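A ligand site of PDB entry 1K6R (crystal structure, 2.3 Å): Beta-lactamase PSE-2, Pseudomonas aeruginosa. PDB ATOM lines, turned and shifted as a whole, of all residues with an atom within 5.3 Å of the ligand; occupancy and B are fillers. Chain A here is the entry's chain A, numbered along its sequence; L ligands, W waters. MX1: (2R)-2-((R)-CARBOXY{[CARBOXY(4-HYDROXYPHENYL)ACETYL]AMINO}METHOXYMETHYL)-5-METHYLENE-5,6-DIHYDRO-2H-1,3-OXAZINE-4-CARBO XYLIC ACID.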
ATOM      1  N   LEU A  46     -18.043   1.988   5.666  1.00  0.00           N
ATOM      2  CA  LEU A  46     -19.147   2.947   5.701  1.00  0.00           C
ATOM      3  C   LEU A  46     -19.155   3.516   7.131  1.00  0.00           C
ATOM      4  O   LEU A  46     -19.165   2.758   8.106  1.00  0.00           O
ATOM      5  CB  LEU A  46     -20.476   2.238   5.427  1.00  0.00           C
ATOM      6  CG  LEU A  46     -21.703   3.138   5.559  1.00  0.00           C
ATOM      7  CD1 LEU A  46     -21.960   3.865   4.247  1.00  0.00           C
ATOM      8  CD2 LEU A  46     -22.906   2.296   5.964  1.00  0.00           C
ATOM      9  N   PRO A  47     -19.159   4.853   7.270  1.00  0.00           N
ATOM     10  CA  PRO A  47     -19.166   5.445   8.619  1.00  0.00           C
ATOM     11  C   PRO A  47     -20.464   5.276   9.404  1.00  0.00           C
ATOM     12  O   PRO A  47     -20.444   5.261  10.634  1.00  0.00           O
ATOM     13  CB  PRO A  47     -18.852   6.911   8.338  1.00  0.00           C
ATOM     14  CG  PRO A  47     -19.503   7.133   6.975  1.00  0.00           C
ATOM     15  CD  PRO A  47     -19.086   5.890   6.225  1.00  0.00           C
ATOM     16  N   ALA A  48     -21.590   5.156   8.707  1.00  0.00           N
ATOM     17  CA  ALA A  48     -22.891   5.036   9.361  1.00  0.00           C
ATOM     18  C   ALA A  48     -23.053   6.213  10.338  1.00  0.00           C
ATOM     19  O   ALA A  48     -22.647   7.335  10.017  1.00  0.00           O
ATOM     20  CB  ALA A  48     -22.996   3.710  10.112  1.00  0.00           C
ATOM     21  N   SER A  49     -23.618   5.958  11.515  1.00  0.00           N
ATOM     22  CA  SER A  49     -23.845   7.018  12.511  1.00  0.00           C
ATOM     23  C   SER A  49     -22.620   7.862  12.892  1.00  0.00           C
ATOM     24  O   SER A  49     -22.783   9.000  13.333  1.00  0.00           O
ATOM     25  CB  SER A  49     -24.446   6.441  13.799  1.00  0.00           C
ATOM     26  OG  SER A  49     -25.763   5.910  13.622  1.00  0.00           O
ATOM     27  N   THR A  50     -21.398   7.344  12.724  1.00  0.00           N
ATOM     28  CA  THR A  50     -20.241   8.159  13.098  1.00  0.00           C
ATOM     29  C   THR A  50     -20.141   9.385  12.191  1.00  0.00           C
ATOM     30  O   THR A  50     -19.476  10.369  12.536  1.00  0.00           O
ATOM     31  CB  THR A  50     -18.885   7.361  13.092  1.00  0.00           C
ATOM     32  OG1 THR A  50     -18.476   7.072  11.746  1.00  0.00           O
ATOM     33  CG2 THR A  50     -19.035   6.050  13.869  1.00  0.00           C
ATOM     34  N   LYS A  52     -22.376  11.384  11.789  1.00  0.00           N
ATOM     35  CA  LYS A  52     -23.158  12.441  12.410  1.00  0.00           C
ATOM     36  C   LYS A  52     -22.262  13.543  12.977  1.00  0.00           C
ATOM     37  O   LYS A  52     -22.712  14.678  13.139  1.00  0.00           O
ATOM     38  CB  LYS A  52     -24.061  11.883  13.526  1.00  0.00           C
ATOM     39  CG  LYS A  52     -25.485  11.503  13.082  1.00  0.00           C
ATOM     40  CD  LYS A  52     -25.554  10.147  12.418  1.00  0.00           C
ATOM     41  CE  LYS A  52     -26.981   9.790  12.017  1.00  0.00           C
ATOM     42  NZ  LYS A  52     -27.056   8.458  11.319  1.00  0.00           N
ATOM     43  N   MET A  81     -37.448   4.916  14.590  1.00  0.00           N
ATOM     44  CA  MET A  81     -37.230   4.521  15.978  1.00  0.00           C
ATOM     45  C   MET A  81     -38.022   5.392  16.942  1.00  0.00           C
ATOM     46  O   MET A  81     -38.087   6.605  16.760  1.00  0.00           O
ATOM     47  CB  MET A  81     -35.736   4.576  16.319  1.00  0.00           C
ATOM     48  CG  MET A  81     -34.919   3.519  15.587  1.00  0.00           C
ATOM     49  SD  MET A  81     -33.209   3.440  16.150  1.00  0.00           S
ATOM     50  CE  MET A  81     -32.390   2.826  14.652  1.00  0.00           C
ATOM     51  N   TRP A  84     -36.795   8.648  18.423  1.00  0.00           N
ATOM     52  CA  TRP A  84     -36.637   9.807  17.544  1.00  0.00           C
ATOM     53  C   TRP A  84     -37.975  10.553  17.440  1.00  0.00           C
ATOM     54  O   TRP A  84     -38.031  11.654  16.888  1.00  0.00           O
ATOM     55  CB  TRP A  84     -36.220   9.390  16.124  1.00  0.00           C
ATOM     56  CG  TRP A  84     -34.971   8.562  16.012  1.00  0.00           C
ATOM     57  CD1 TRP A  84     -33.984   8.421  16.954  1.00  0.00           C
ATOM     58  CD2 TRP A  84     -34.554   7.788  14.874  1.00  0.00           C
ATOM     59  NE1 TRP A  84     -32.989   7.610  16.466  1.00  0.00           N
ATOM     60  CE2 TRP A  84     -33.317   7.208  15.203  1.00  0.00           C
ATOM     61  CE3 TRP A  84     -35.129   7.536  13.617  1.00  0.00           C
ATOM     62  CZ2 TRP A  84     -32.621   6.375  14.311  1.00  0.00           C
ATOM     63  CZ3 TRP A  84     -34.439   6.710  12.731  1.00  0.00           C
ATOM     64  CH2 TRP A  84     -33.194   6.135  13.079  1.00  0.00           C
ATOM     65  N   SER A  97     -28.662   8.936  17.506  1.00  0.00           N
ATOM     66  CA  SER A  97     -28.507   8.858  16.053  1.00  0.00           C
ATOM     67  C   SER A  97     -29.811   9.105  15.274  1.00  0.00           C
ATOM     68  O   SER A  97     -30.169   8.332  14.386  1.00  0.00           O
ATOM     69  CB  SER A  97     -27.948   7.488  15.658  1.00  0.00           C
ATOM     70  OG  SER A  97     -26.655   7.276  16.219  1.00  0.00           O
ATOM     71  N   VAL A  99     -31.628   9.752  12.660  1.00  0.00           N
ATOM     72  CA  VAL A  99     -31.482   9.843  11.214  1.00  0.00           C
ATOM     73  C   VAL A  99     -32.252  10.957  10.521  1.00  0.00           C
ATOM     74  O   VAL A  99     -31.669  11.761   9.800  1.00  0.00           O
ATOM     75  CB  VAL A  99     -31.841   8.499  10.528  1.00  0.00           C
ATOM     76  CG1 VAL A  99     -31.905   8.674   9.016  1.00  0.00           C
ATOM     77  CG2 VAL A  99     -30.803   7.466  10.874  1.00  0.00           C
ATOM     78  N   TRP A 136     -24.144   8.315   3.708  1.00  0.00           N
ATOM     79  CA  TRP A 136     -23.416   7.794   4.854  1.00  0.00           C
ATOM     80  C   TRP A 136     -24.157   6.633   5.531  1.00  0.00           C
ATOM     81  O   TRP A 136     -23.623   6.001   6.434  1.00  0.00           O
ATOM     82  CB  TRP A 136     -23.168   8.913   5.868  1.00  0.00           C
ATOM     83  CG  TRP A 136     -24.369   9.293   6.715  1.00  0.00           C
ATOM     84  CD1 TRP A 136     -24.705   8.781   7.928  1.00  0.00           C
ATOM     85  CD2 TRP A 136     -25.358  10.293   6.406  1.00  0.00           C
ATOM     86  NE1 TRP A 136     -25.846   9.397   8.412  1.00  0.00           N
ATOM     87  CE2 TRP A 136     -26.255  10.325   7.490  1.00  0.00           C
ATOM     88  CE3 TRP A 136     -25.566  11.152   5.317  1.00  0.00           C
ATOM     89  CZ2 TRP A 136     -27.360  11.198   7.527  1.00  0.00           C
ATOM     90  CZ3 TRP A 136     -26.652  12.013   5.350  1.00  0.00           C
ATOM     91  CH2 TRP A 136     -27.534  12.031   6.449  1.00  0.00           C
ATOM     92  N   LEU A 137     -25.380   6.377   5.081  1.00  0.00           N
ATOM     93  CA  LEU A 137     -26.196   5.290   5.649  1.00  0.00           C
ATOM     94  C   LEU A 137     -26.148   4.021   4.814  1.00  0.00           C
ATOM     95  O   LEU A 137     -26.216   2.916   5.344  1.00  0.00           O
ATOM     96  CB  LEU A 137     -27.663   5.726   5.782  1.00  0.00           C
ATOM     97  CG  LEU A 137     -27.994   6.939   6.642  1.00  0.00           C
ATOM     98  CD1 LEU A 137     -29.485   7.260   6.541  1.00  0.00           C
ATOM     99  CD2 LEU A 137     -27.618   6.648   8.091  1.00  0.00           C
ATOM    100  N   GLU A 138     -26.044   4.182   3.486  1.00  0.00           N
ATOM    101  CA  GLU A 138     -26.032   3.046   2.576  1.00  0.00           C
ATOM    102  C   GLU A 138     -25.305   3.346   1.269  1.00  0.00           C
ATOM    103  O   GLU A 138     -25.371   2.570   0.321  1.00  0.00           O
ATOM    104  CB  GLU A 138     -27.476   2.645   2.244  1.00  0.00           C
ATOM    105  CG  GLU A 138     -28.269   3.762   1.559  1.00  0.00           C
ATOM    106  CD  GLU A 138     -29.607   3.309   1.011  1.00  0.00           C
ATOM    107  OE1 GLU A 138     -29.635   2.710  -0.091  1.00  0.00           O
ATOM    108  OE2 GLU A 138     -30.633   3.541   1.675  1.00  0.00           O
ATOM    109  N   THR A 188     -20.871   6.058  18.437  1.00  0.00           N
ATOM    110  CA  THR A 188     -20.992   4.695  17.927  1.00  0.00           C
ATOM    111  C   THR A 188     -21.619   4.707  16.543  1.00  0.00           C
ATOM    112  O   THR A 188     -22.204   5.706  16.127  1.00  0.00           O
ATOM    113  CB  THR A 188     -21.867   3.818  18.831  1.00  0.00           C
ATOM    114  OG1 THR A 188     -23.116   4.474  19.076  1.00  0.00           O
ATOM    115  CG2 THR A 188     -21.163   3.542  20.146  1.00  0.00           C
ATOM    116  N   GLY A 189     -21.482   3.592  15.842  1.00  0.00           N
ATOM    117  CA  GLY A 189     -22.049   3.449  14.511  1.00  0.00           C
ATOM    118  C   GLY A 189     -22.263   1.975  14.205  1.00  0.00           C
ATOM    119  O   GLY A 189     -21.603   1.120  14.768  1.00  0.00           O
ATOM    120  N   PHE A 190     -23.199   1.697  13.298  1.00  0.00           N
ATOM    121  CA  PHE A 190     -23.521   0.326  12.927  1.00  0.00           C
ATOM    122  C   PHE A 190     -24.153   0.374  11.534  1.00  0.00           C
ATOM    123  O   PHE A 190     -25.185   0.991  11.358  1.00  0.00           O
ATOM    124  CB  PHE A 190     -24.495  -0.241  13.973  1.00  0.00           C
ATOM    125  CG  PHE A 190     -25.108  -1.560  13.609  1.00  0.00           C
ATOM    126  CD1 PHE A 190     -24.319  -2.631  13.197  1.00  0.00           C
ATOM    127  CD2 PHE A 190     -26.486  -1.758  13.741  1.00  0.00           C
ATOM    128  CE1 PHE A 190     -24.899  -3.869  12.910  1.00  0.00           C
ATOM    129  CE2 PHE A 190     -27.072  -2.990  13.459  1.00  0.00           C
ATOM    130  CZ  PHE A 190     -26.284  -4.046  13.049  1.00  0.00           C
ATOM    131  N   SER A 191     -23.539  -0.264  10.541  1.00  0.00           N
ATOM    132  CA  SER A 191     -24.085  -0.217   9.191  1.00  0.00           C
ATOM    133  C   SER A 191     -25.260  -1.165   8.981  1.00  0.00           C
ATOM    134  O   SER A 191     -26.044  -0.988   8.059  1.00  0.00           O
ATOM    135  CB  SER A 191     -22.994  -0.526   8.162  1.00  0.00           C
ATOM    136  OG  SER A 191     -22.566  -1.874   8.248  1.00  0.00           O
ATOM    137  N   GLY A 192     -25.392  -2.169   9.850  1.00  0.00           N
ATOM    138  CA  GLY A 192     -26.477  -3.121   9.707  1.00  0.00           C
ATOM    139  C   GLY A 192     -25.940  -4.532   9.761  1.00  0.00           C
ATOM    140  O   GLY A 192     -24.737  -4.712   9.906  1.00  0.00           O
ATOM    141  N   TRP A 203     -18.927   0.423  14.748  1.00  0.00           N
ATOM    142  CA  TRP A 203     -17.919   1.407  15.122  1.00  0.00           C
ATOM    143  C   TRP A 203     -18.022   1.967  16.529  1.00  0.00           C
ATOM    144  O   TRP A 203     -19.085   1.947  17.171  1.00  0.00           O
ATOM    145  CB  TRP A 203     -17.995   2.654  14.238  1.00  0.00           C
ATOM    146  CG  TRP A 203     -17.618   2.579  12.787  1.00  0.00           C
ATOM    147  CD1 TRP A 203     -18.446   2.378  11.729  1.00  0.00           C
ATOM    148  CD2 TRP A 203     -16.326   2.896  12.222  1.00  0.00           C
ATOM    149  NE1 TRP A 203     -17.785   2.566  10.548  1.00  0.00           N
ATOM    150  CE2 TRP A 203     -16.479   2.886  10.815  1.00  0.00           C
ATOM    151  CE3 TRP A 203     -15.079   3.189  12.770  1.00  0.00           C
ATOM    152  CZ2 TRP A 203     -15.413   3.158   9.955  1.00  0.00           C
ATOM    153  CZ3 TRP A 203     -14.009   3.468  11.906  1.00  0.00           C
ATOM    154  CH2 TRP A 203     -14.196   3.454  10.504  1.00  0.00           C
ATOM    155  N   GLU A 226     -27.244  -8.238  15.301  1.00  0.00           N
ATOM    156  CA  GLU A 226     -27.372  -7.115  16.208  1.00  0.00           C
ATOM    157  C   GLU A 226     -27.093  -7.454  17.676  1.00  0.00           C
ATOM    158  O   GLU A 226     -26.880  -6.562  18.492  1.00  0.00           O
ATOM    159  CB  GLU A 226     -28.762  -6.512  16.056  1.00  0.00           C
ATOM    160  CG  GLU A 226     -28.862  -5.045  16.429  1.00  0.00           C
ATOM    161  CD  GLU A 226     -30.134  -4.400  15.916  1.00  0.00           C
ATOM    162  OE1 GLU A 226     -30.300  -3.172  16.106  1.00  0.00           O
ATOM    163  OE2 GLU A 226     -30.973  -5.129  15.338  1.00  0.00           O
ATOM    164  N   LEU A 229     -23.544  -6.143  19.130  1.00  0.00           N
ATOM    165  CA  LEU A 229     -23.202  -4.744  19.402  1.00  0.00           C
ATOM    166  C   LEU A 229     -22.412  -4.463  20.682  1.00  0.00           C
ATOM    167  O   LEU A 229     -21.458  -3.681  20.660  1.00  0.00           O
ATOM    168  CB  LEU A 229     -24.465  -3.876  19.379  1.00  0.00           C
ATOM    169  CG  LEU A 229     -24.944  -3.335  18.023  1.00  0.00           C
ATOM    170  CD1 LEU A 229     -23.788  -2.693  17.284  1.00  0.00           C
ATOM    171  CD2 LEU A 229     -25.534  -4.447  17.195  1.00  0.00           C
ATOM    172  N   ARG A 232     -18.750  -4.008  20.545  1.00  0.00           N
ATOM    173  CA  ARG A 232     -18.254  -2.769  19.955  1.00  0.00           C
ATOM    174  C   ARG A 232     -17.676  -1.794  20.994  1.00  0.00           C
ATOM    175  O   ARG A 232     -16.772  -1.003  20.683  1.00  0.00           O
ATOM    176  CB  ARG A 232     -19.377  -2.133  19.134  1.00  0.00           C
ATOM    177  CG  ARG A 232     -19.096  -0.760  18.602  1.00  0.00           C
ATOM    178  CD  ARG A 232     -19.561   0.281  19.596  1.00  0.00           C
ATOM    179  NE  ARG A 232     -20.970   0.108  19.944  1.00  0.00           N
ATOM    180  CZ  ARG A 232     -21.977   0.097  19.074  1.00  0.00           C
ATOM    181  NH1 ARG A 232     -21.750   0.247  17.784  1.00  0.00           N
ATOM    182  NH2 ARG A 232     -23.230  -0.031  19.510  1.00  0.00           N
HETATM  183  O4  MX1 L   1     -24.859   1.978  18.340  1.00  0.00           O
HETATM  184  C7  MX1 L   1     -24.918   1.789  17.104  1.00  0.00           C
HETATM  185  O3  MX1 L   1     -23.903   1.415  16.491  1.00  0.00           O
HETATM  186  C4  MX1 L   1     -26.204   1.996  16.390  1.00  0.00           C
HETATM  187  N1  MX1 L   1     -26.280   3.139  15.546  1.00  0.00           N
HETATM  188  C5  MX1 L   1     -27.248   1.124  16.558  1.00  0.00           C
HETATM  189  C8  MX1 L   1     -27.205  -0.067  17.418  1.00  0.00           C
HETATM  190  C6  MX1 L   1     -28.516   1.393  15.814  1.00  0.00           C
HETATM  191  O2  MX1 L   1     -28.331   2.194  14.616  1.00  0.00           O
HETATM  192  C3  MX1 L   1     -27.524   3.379  14.821  1.00  0.00           C
HETATM  193  C2  MX1 L   1     -27.336   4.008  13.351  1.00  0.00           C
HETATM  194  C1  MX1 L   1     -25.870   4.587  13.288  1.00  0.00           C
HETATM  195  O31 MX1 L   1     -24.854   3.926  13.103  1.00  0.00           O
HETATM  196  O5  MX1 L   1     -28.408   4.979  13.372  1.00  0.00           O
HETATM  197  C9  MX1 L   1     -28.318   6.136  12.567  1.00  0.00           C
HETATM  198  N2  MX1 L   1     -27.512   2.969  12.328  1.00  0.00           N
HETATM  199  C10 MX1 L   1     -27.265   3.121  10.966  1.00  0.00           C
HETATM  200  O6  MX1 L   1     -26.793   4.175  10.477  1.00  0.00           O
HETATM  201  C11 MX1 L   1     -27.575   1.934  10.048  1.00  0.00           C
HETATM  202  C12 MX1 L   1     -27.626   2.403   8.618  1.00  0.00           C
HETATM  203  O8  MX1 L   1     -28.700   2.777   8.103  1.00  0.00           O
HETATM  204  O7  MX1 L   1     -26.573   2.425   7.944  1.00  0.00           O
HETATM  205  C13 MX1 L   1     -28.844   1.212  10.472  1.00  0.00           C
HETATM  206  C14 MX1 L   1     -30.100   1.811  10.362  1.00  0.00           C
HETATM  207  C18 MX1 L   1     -28.779  -0.091  10.977  1.00  0.00           C
HETATM  208  C17 MX1 L   1     -29.926  -0.782  11.372  1.00  0.00           C
HETATM  209  C16 MX1 L   1     -31.161  -0.173  11.256  1.00  0.00           C
HETATM  210  O9  MX1 L   1     -32.305  -0.843  11.649  1.00  0.00           O
HETATM  211  C15 MX1 L   1     -31.267   1.125  10.747  1.00  0.00           C
HETATM  212  O   HOH W   1     -30.311   2.449   6.163  1.00  0.00           O
HETATM  213  O   HOH W   2     -30.864  -0.772  14.949  1.00  0.00           O
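N of Ser 49 sits close to O31 of the ligand (2.9 Å).
The side-chain hydroxyl of Ser 49 is covalently linked to a carbon (C1) of the ligand, at 1.4 Å.
O of Leu 137 lies close to O7 of the ligand, 2.7 Å away.
NH1 of Arg 232 is in salt-bridge range of O3 of the ligand, 2.8 Å away.
An oxygen (O31) of the ligand is in hydrogen-bond range of the backbone NH (N) of Phe 190, at 2.8 Å.
The backbone carbonyl oxygen (O) of Phe 190 sits close to a nitrogen (N2) of the ligand (3.2 Å).
An oxygen (O3) of the ligand lies close to the backbone NH of Gly 189 (3.3 Å).
O3 of the ligand lies close to O of Gly 189 (2.9 Å).
OG1 of Thr 188 sits at hydrogen-bond distance from O4 of the ligand (3.1 Å).
OG of Ser 49 lies within hydrogen-bond range of OG of Ser 97, at 3.1 Å.
The backbone carbonyl oxygen of Gly 189 sits at hydrogen-bond distance from the guanidinium group of Arg 232, at 3.1 Å.
O of Trp 203 lies close to NH1 of Arg 232, 3.2 Å away.
N of Trp 203 sits at hydrogen-bond distance from O of Gly 189 (2.8 Å).
N of Ala 48 sits at hydrogen-bond distance from O of Trp 136, at 3.2 Å.
O of Ser 191 sits close to O7 of the ligand, at 3.5 Å.
Ala 48 touches the ligand.
Lys 52 touches the ligand.
Ser 97 touches the ligand.
Val 99 touches the ligand.
Hydrophobic or aromatic side chains that line the ligand: Ala 48, Val 99, Leu 137 and Phe 190.
The nearest printed residue that does not touch the ligand is Gly 192 (4.01 Å).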
